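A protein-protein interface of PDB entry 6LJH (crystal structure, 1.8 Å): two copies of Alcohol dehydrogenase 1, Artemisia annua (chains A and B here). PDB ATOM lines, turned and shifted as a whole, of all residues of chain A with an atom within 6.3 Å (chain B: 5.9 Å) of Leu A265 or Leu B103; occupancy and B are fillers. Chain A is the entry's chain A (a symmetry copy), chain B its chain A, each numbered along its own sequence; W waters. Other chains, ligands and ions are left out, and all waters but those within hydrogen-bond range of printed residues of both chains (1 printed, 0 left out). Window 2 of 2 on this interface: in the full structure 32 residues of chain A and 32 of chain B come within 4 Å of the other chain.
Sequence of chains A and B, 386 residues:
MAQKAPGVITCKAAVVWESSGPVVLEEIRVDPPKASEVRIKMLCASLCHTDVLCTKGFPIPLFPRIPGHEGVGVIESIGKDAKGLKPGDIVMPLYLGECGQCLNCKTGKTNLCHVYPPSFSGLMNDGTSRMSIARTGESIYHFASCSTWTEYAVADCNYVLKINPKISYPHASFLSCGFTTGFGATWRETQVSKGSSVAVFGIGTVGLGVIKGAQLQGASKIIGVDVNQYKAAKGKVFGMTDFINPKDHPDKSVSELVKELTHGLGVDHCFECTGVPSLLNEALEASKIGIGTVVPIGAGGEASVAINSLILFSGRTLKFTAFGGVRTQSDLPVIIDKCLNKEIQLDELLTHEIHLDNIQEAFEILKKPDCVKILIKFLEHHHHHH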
ATOM      1  N   VAL A 258       5.573 -22.257  12.796  1.00  0.00           N
ATOM      2  CA  VAL A 258       5.507 -23.141  13.957  1.00  0.00           C
ATOM      3  C   VAL A 258       5.290 -22.336  15.228  1.00  0.00           C
ATOM      4  O   VAL A 258       4.511 -22.728  16.111  1.00  0.00           O
ATOM      5  CB  VAL A 258       6.779 -24.008  14.055  1.00  0.00           C
ATOM      6  CG1 VAL A 258       6.804 -24.781  15.383  1.00  0.00           C
ATOM      7  CG2 VAL A 258       6.846 -24.979  12.881  1.00  0.00           C
ATOM      8  N   LYS A 259       5.979 -21.201  15.349  1.00  0.00           N
ATOM      9  CA  LYS A 259       5.801 -20.369  16.529  1.00  0.00           C
ATOM     10  C   LYS A 259       4.372 -19.856  16.632  1.00  0.00           C
ATOM     11  O   LYS A 259       3.841 -19.744  17.738  1.00  0.00           O
ATOM     12  CB  LYS A 259       6.806 -19.216  16.505  1.00  0.00           C
ATOM     13  CG  LYS A 259       8.208 -19.690  16.827  1.00  0.00           C
ATOM     14  CD  LYS A 259       9.123 -18.517  17.116  1.00  0.00           C
ATOM     15  CE  LYS A 259      10.015 -18.237  15.947  1.00  0.00           C
ATOM     16  NZ  LYS A 259      10.878 -17.049  16.211  1.00  0.00           N
ATOM     17  N   THR A 262       2.407 -22.289  18.647  1.00  0.00           N
ATOM     18  CA  THR A 262       2.977 -22.681  19.934  1.00  0.00           C
ATOM     19  C   THR A 262       3.185 -21.472  20.826  1.00  0.00           C
ATOM     20  O   THR A 262       4.156 -21.403  21.589  1.00  0.00           O
ATOM     21  CB  THR A 262       4.296 -23.436  19.749  1.00  0.00           C
ATOM     22  OG1 THR A 262       5.171 -22.679  18.905  1.00  0.00           O
ATOM     23  CG2 THR A 262       4.040 -24.802  19.119  1.00  0.00           C
ATOM     24  N   HIS A 263       2.278 -20.496  20.736  1.00  0.00           N
ATOM     25  CA  HIS A 263       2.289 -19.330  21.623  1.00  0.00           C
ATOM     26  C   HIS A 263       3.573 -18.519  21.492  1.00  0.00           C
ATOM     27  O   HIS A 263       4.040 -17.916  22.461  1.00  0.00           O
ATOM     28  CB  HIS A 263       2.060 -19.761  23.072  1.00  0.00           C
ATOM     29  CG  HIS A 263       0.792 -20.529  23.268  1.00  0.00           C
ATOM     30  ND1 HIS A 263       0.771 -21.878  23.551  1.00  0.00           N
ATOM     31  CD2 HIS A 263      -0.505 -20.142  23.192  1.00  0.00           C
ATOM     32  CE1 HIS A 263      -0.480 -22.286  23.651  1.00  0.00           C
ATOM     33  NE2 HIS A 263      -1.274 -21.252  23.439  1.00  0.00           N
ATOM     34  N   GLY A 264       4.140 -18.474  20.288  1.00  0.00           N
ATOM     35  CA  GLY A 264       5.379 -17.771  20.041  1.00  0.00           C
ATOM     36  C   GLY A 264       6.627 -18.444  20.573  1.00  0.00           C
ATOM     37  O   GLY A 264       7.713 -17.878  20.435  1.00  0.00           O
ATOM     38  N   LEU A 265       6.513 -19.624  21.183  1.00  0.00           N
ATOM     39  CA  LEU A 265       7.653 -20.262  21.840  1.00  0.00           C
ATOM     40  C   LEU A 265       8.396 -21.262  20.961  1.00  0.00           C
ATOM     41  O   LEU A 265       9.597 -21.482  21.173  1.00  0.00           O
ATOM     42  CB  LEU A 265       7.194 -20.999  23.099  1.00  0.00           C
ATOM     43  CG  LEU A 265       6.618 -20.193  24.267  1.00  0.00           C
ATOM     44  CD1 LEU A 265       5.885 -21.129  25.203  1.00  0.00           C
ATOM     45  CD2 LEU A 265       7.719 -19.463  24.998  1.00  0.00           C
ATOM     46  N   GLY A 266       7.719 -21.901  20.009  1.00  0.00           N
ATOM     47  CA  GLY A 266       8.301 -23.047  19.329  1.00  0.00           C
ATOM     48  C   GLY A 266       8.009 -24.351  20.059  1.00  0.00           C
ATOM     49  O   GLY A 266       7.301 -24.392  21.070  1.00  0.00           O
ATOM     50  N   VAL A 267       8.584 -25.449  19.546  1.00  0.00           N
ATOM     51  CA  VAL A 267       8.287 -26.788  20.059  1.00  0.00           C
ATOM     52  C   VAL A 267       9.413 -27.288  20.955  1.00  0.00           C
ATOM     53  O   VAL A 267      10.556 -26.835  20.883  1.00  0.00           O
ATOM     54  CB  VAL A 267       8.028 -27.811  18.924  1.00  0.00           C
ATOM     55  CG1 VAL A 267       6.763 -27.441  18.157  1.00  0.00           C
ATOM     56  CG2 VAL A 267       9.210 -27.869  17.989  1.00  0.00           C
ATOM     57  N   GLU A 285      15.364 -22.696  14.781  1.00  0.00           N
ATOM     58  CA  GLU A 285      14.553 -21.528  15.122  1.00  0.00           C
ATOM     59  C   GLU A 285      13.143 -21.919  15.530  1.00  0.00           C
ATOM     60  O   GLU A 285      12.487 -21.173  16.263  1.00  0.00           O
ATOM     61  CB  GLU A 285      14.478 -20.552  13.947  1.00  0.00           C
ATOM     62  CG  GLU A 285      15.806 -20.018  13.469  1.00  0.00           C
ATOM     63  CD  GLU A 285      16.324 -18.894  14.339  1.00  0.00           C
ATOM     64  OE1 GLU A 285      15.726 -18.621  15.405  1.00  0.00           O
ATOM     65  OE2 GLU A 285      17.329 -18.269  13.950  1.00  0.00           O
ATOM     66  N   ALA A 286      12.648 -23.059  15.052  1.00  0.00           N
ATOM     67  CA  ALA A 286      11.316 -23.510  15.434  1.00  0.00           C
ATOM     68  C   ALA A 286      11.278 -24.205  16.787  1.00  0.00           C
ATOM     69  O   ALA A 286      10.184 -24.439  17.308  1.00  0.00           O
ATOM     70  CB  ALA A 286      10.744 -24.463  14.377  1.00  0.00           C
ATOM     71  N   SER A 287      12.417 -24.565  17.361  1.00  0.00           N
ATOM     72  CA  SER A 287      12.408 -25.186  18.676  1.00  0.00           C
ATOM     73  C   SER A 287      12.588 -24.118  19.757  1.00  0.00           C
ATOM     74  O   SER A 287      13.078 -23.018  19.503  1.00  0.00           O
ATOM     75  CB  SER A 287      13.515 -26.250  18.779  1.00  0.00           C
ATOM     76  OG  SER A 287      14.789 -25.630  18.727  1.00  0.00           O
ATOM     77  N   LYS A 288      12.183 -24.463  20.980  1.00  0.00           N
ATOM     78  CA  LYS A 288      12.194 -23.498  22.080  1.00  0.00           C
ATOM     79  C   LYS A 288      13.603 -23.049  22.429  1.00  0.00           C
ATOM     80  O   LYS A 288      14.526 -23.864  22.533  1.00  0.00           O
ATOM     81  CB  LYS A 288      11.555 -24.105  23.326  1.00  0.00           C
ATOM     82  CG  LYS A 288      10.051 -24.306  23.207  1.00  0.00           C
ATOM     83  CD  LYS A 288       9.517 -24.985  24.461  1.00  0.00           C
ATOM     84  CE  LYS A 288       8.009 -25.228  24.349  1.00  0.00           C
ATOM     85  NZ  LYS A 288       7.486 -26.007  25.531  1.00  0.00           N
ATOM     86  N   ILE A 289      13.756 -21.742  22.648  1.00  0.00           N
ATOM     87  CA  ILE A 289      14.974 -21.241  23.280  1.00  0.00           C
ATOM     88  C   ILE A 289      15.203 -21.927  24.623  1.00  0.00           C
ATOM     89  O   ILE A 289      14.275 -22.116  25.417  1.00  0.00           O
ATOM     90  CB  ILE A 289      14.875 -19.714  23.438  1.00  0.00           C
ATOM     91  CG1 ILE A 289      14.860 -19.048  22.061  1.00  0.00           C
ATOM     92  CG2 ILE A 289      16.044 -19.147  24.270  1.00  0.00           C
ATOM     93  CD1 ILE A 289      14.369 -17.608  22.084  1.00  0.00           C
ATOM     94  N   ILE A 291      15.404 -24.780  26.017  1.00  0.00           N
ATOM     95  CA  ILE A 291      14.998 -26.141  26.347  1.00  0.00           C
ATOM     96  C   ILE A 291      14.616 -26.965  25.126  1.00  0.00           C
ATOM     97  O   ILE A 291      14.242 -28.132  25.272  1.00  0.00           O
ATOM     98  CB  ILE A 291      13.850 -26.146  27.383  1.00  0.00           C
ATOM     99  CG1 ILE A 291      12.585 -25.495  26.814  1.00  0.00           C
ATOM    100  CG2 ILE A 291      14.293 -25.442  28.685  1.00  0.00           C
ATOM    101  CD1 ILE A 291      11.356 -25.604  27.763  1.00  0.00           C
ATOM    102  N   ARG A 316      19.775 -24.235  22.815  1.00  0.00           N
ATOM    103  CA  ARG A 316      19.155 -25.408  22.219  1.00  0.00           C
ATOM    104  C   ARG A 316      20.140 -26.571  22.134  1.00  0.00           C
ATOM    105  O   ARG A 316      21.352 -26.397  22.178  1.00  0.00           O
ATOM    106  CB  ARG A 316      18.627 -25.064  20.823  1.00  0.00           C
ATOM    107  CG  ARG A 316      17.512 -24.023  20.861  1.00  0.00           C
ATOM    108  CD  ARG A 316      17.205 -23.530  19.479  1.00  0.00           C
ATOM    109  NE  ARG A 316      16.016 -22.673  19.432  1.00  0.00           N
ATOM    110  CZ  ARG A 316      16.044 -21.406  19.040  1.00  0.00           C
ATOM    111  NH1 ARG A 316      17.199 -20.846  18.706  1.00  0.00           N
ATOM    112  NH2 ARG A 316      14.925 -20.703  18.974  1.00  0.00           N
ATOM    113  N   GLN B 101      10.210 -17.383  37.627  1.00  0.00           N
ATOM    114  CA  GLN B 101       8.785 -17.671  37.502  1.00  0.00           C
ATOM    115  C   GLN B 101       8.328 -17.984  36.085  1.00  0.00           C
ATOM    116  O   GLN B 101       7.226 -18.527  35.930  1.00  0.00           O
ATOM    117  CB  GLN B 101       7.950 -16.485  38.019  1.00  0.00           C
ATOM    118  CG  GLN B 101       8.041 -16.235  39.527  1.00  0.00           C
ATOM    119  CD  GLN B 101       7.464 -17.381  40.360  1.00  0.00           C
ATOM    120  OE1 GLN B 101       6.481 -18.022  39.971  1.00  0.00           O
ATOM    121  NE2 GLN B 101       8.075 -17.637  41.514  1.00  0.00           N
ATOM    122  N   CYS B 102       9.103 -17.640  35.053  1.00  0.00           N
ATOM    123  CA  CYS B 102       8.678 -17.857  33.677  1.00  0.00           C
ATOM    124  C   CYS B 102       8.804 -19.337  33.314  1.00  0.00           C
ATOM    125  O   CYS B 102       9.302 -20.156  34.087  1.00  0.00           O
ATOM    126  CB  CYS B 102       9.497 -16.991  32.710  1.00  0.00           C
ATOM    127  SG  CYS B 102      11.240 -17.533  32.525  1.00  0.00           S
ATOM    128  N   LEU B 103       8.346 -19.681  32.109  1.00  0.00           N
ATOM    129  CA  LEU B 103       8.369 -21.083  31.697  1.00  0.00           C
ATOM    130  C   LEU B 103       9.786 -21.637  31.692  1.00  0.00           C
ATOM    131  O   LEU B 103      10.019 -22.763  32.150  1.00  0.00           O
ATOM    132  CB  LEU B 103       7.749 -21.243  30.316  1.00  0.00           C
ATOM    133  CG  LEU B 103       6.250 -20.987  30.289  1.00  0.00           C
ATOM    134  CD1 LEU B 103       5.817 -20.930  28.847  1.00  0.00           C
ATOM    135  CD2 LEU B 103       5.510 -22.084  31.049  1.00  0.00           C
ATOM    136  N   ASN B 104      10.749 -20.860  31.196  1.00  0.00           N
ATOM    137  CA  ASN B 104      12.122 -21.370  31.151  1.00  0.00           C
ATOM    138  C   ASN B 104      12.727 -21.498  32.551  1.00  0.00           C
ATOM    139  O   ASN B 104      13.386 -22.501  32.857  1.00  0.00           O
ATOM    140  CB  ASN B 104      12.984 -20.477  30.250  1.00  0.00           C
ATOM    141  CG  ASN B 104      13.110 -21.038  28.837  1.00  0.00           C
ATOM    142  OD1 ASN B 104      12.459 -22.035  28.495  1.00  0.00           O
ATOM    143  ND2 ASN B 104      13.947 -20.409  28.009  1.00  0.00           N
ATOM    144  N   CYS B 105      12.511 -20.501  33.422  1.00  0.00           N
ATOM    145  CA  CYS B 105      13.071 -20.564  34.772  1.00  0.00           C
ATOM    146  C   CYS B 105      12.497 -21.747  35.547  1.00  0.00           C
ATOM    147  O   CYS B 105      13.216 -22.428  36.291  1.00  0.00           O
ATOM    148  CB  CYS B 105      12.801 -19.250  35.520  1.00  0.00           C
ATOM    149  SG  CYS B 105      13.895 -17.840  35.031  1.00  0.00           S
ATOM    150  N   LYS B 106      11.207 -22.028  35.359  1.00  0.00           N
ATOM    151  CA  LYS B 106      10.590 -23.111  36.122  1.00  0.00           C
ATOM    152  C   LYS B 106      11.174 -24.479  35.763  1.00  0.00           C
ATOM    153  O   LYS B 106      11.167 -25.378  36.611  1.00  0.00           O
ATOM    154  CB  LYS B 106       9.076 -23.094  35.926  1.00  0.00           C
ATOM    155  CG  LYS B 106       8.406 -21.891  36.604  1.00  0.00           C
ATOM    156  CD  LYS B 106       7.080 -22.279  37.257  1.00  0.00           C
ATOM    157  CE  LYS B 106       6.711 -21.344  38.415  1.00  0.00           C
ATOM    158  NZ  LYS B 106       5.665 -20.336  38.052  1.00  0.00           N
ATOM    159  N   THR B 107      11.713 -24.658  34.543  1.00  0.00           N
ATOM    160  CA  THR B 107      12.257 -25.965  34.171  1.00  0.00           C
ATOM    161  C   THR B 107      13.513 -26.320  34.951  1.00  0.00           C
ATOM    162  O   THR B 107      13.835 -27.504  35.073  1.00  0.00           O
ATOM    163  CB  THR B 107      12.616 -26.051  32.678  1.00  0.00           C
ATOM    164  OG1 THR B 107      13.756 -25.224  32.410  1.00  0.00           O
ATOM    165  CG2 THR B 107      11.438 -25.682  31.776  1.00  0.00           C
ATOM    166  N   HIS B 114      12.832 -15.813  30.100  1.00  0.00           N
ATOM    167  CA  HIS B 114      11.960 -15.110  29.159  1.00  0.00           C
ATOM    168  C   HIS B 114      11.747 -13.657  29.553  1.00  0.00           C
ATOM    169  O   HIS B 114      11.497 -12.817  28.687  1.00  0.00           O
ATOM    170  CB  HIS B 114      10.591 -15.782  29.082  1.00  0.00           C
ATOM    171  CG  HIS B 114      10.605 -17.129  28.436  1.00  0.00           C
ATOM    172  ND1 HIS B 114       9.599 -18.054  28.639  1.00  0.00           N
ATOM    173  CD2 HIS B 114      11.492 -17.711  27.592  1.00  0.00           C
ATOM    174  CE1 HIS B 114       9.874 -19.155  27.959  1.00  0.00           C
ATOM    175  NE2 HIS B 114      11.009 -18.967  27.304  1.00  0.00           N
HETATM  176  O   HOH W   1      11.652 -21.075  25.378  1.00  0.00           O
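Of chain B, only Leu B103 (3.7 Å) and His B114 (3.7 Å) come within 4 Å of Leu A265. Leu B103 touches just one residue of chain A: Leu A265 (3.7 Å). Of the printed residues of chain A, Asn B104 touches Ile A289 (3.1 Å) and Ile A291 (3.8 Å). Of the printed residues of chain B, Ile A291 touches Asn B104 and Thr B107. Printed residues of chain B within 4 Å of Ile A289: Asn B104 (3.1 Å). Gly A266 touches none of the printed residues of chain B. The nearest residue of chain A that does not touch Leu B103 is Ile A291 (5.4 Å). The nearest printed residue of chain A that does not touch Asn B104 is Lys A288 (5.6 Å).
Printed residues of chain B that touch a printed residue of chain A: Leu B103, Asn B104, Thr B107 and His B114. Of the 15 printed residues of chain A, 3 touch a printed residue of chain B. Printed residues of chain A that touch a printed residue of chain B: Leu A265, Ile A289 and Ile A291.
SG of Cys B102 sits close to N of His B114 (3.4 Å). The side-chain sulfur (SG) of Cys B102 lies close to the backbone NH (N) of Asn B104 (3.6 Å). The side-chain amide nitrogen of Asn B104 sits close to a ring nitrogen (NE2) of His B114, 3.3 Å away. The backbone carbonyl oxygen (O) of Asn B104 lies within hydrogen-bond range of the side-chain hydroxyl (OG1) of Thr B107, 2.8 Å away.
Water W1 lies within hydrogen-bond range of the backbone carbonyl oxygen of Ile A289 (2.8 Å), a ring nitrogen (NE2) of His B114 (2.9 Å) and the side-chain amide oxygen of Asn B104 (3.4 Å).
The backbone carbonyl oxygen (O) of Ile A289 lies within hydrogen-bond range of the side-chain amide nitrogen (ND2) of Asn B104 (3.1 Å).
Leu B103 touches Leu A265. Leu A265 touches His B114 (CD2 to CE1, 3.7 Å). CD1 of Ile A291 touches OD1 of Asn B104, 3.8 Å away. Ile A291 touches Thr B107.
No position is printed for both chains. Of the 5 pairs that touch across the chains among the printed residues, none has its exchanged pair printed and touching as well.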
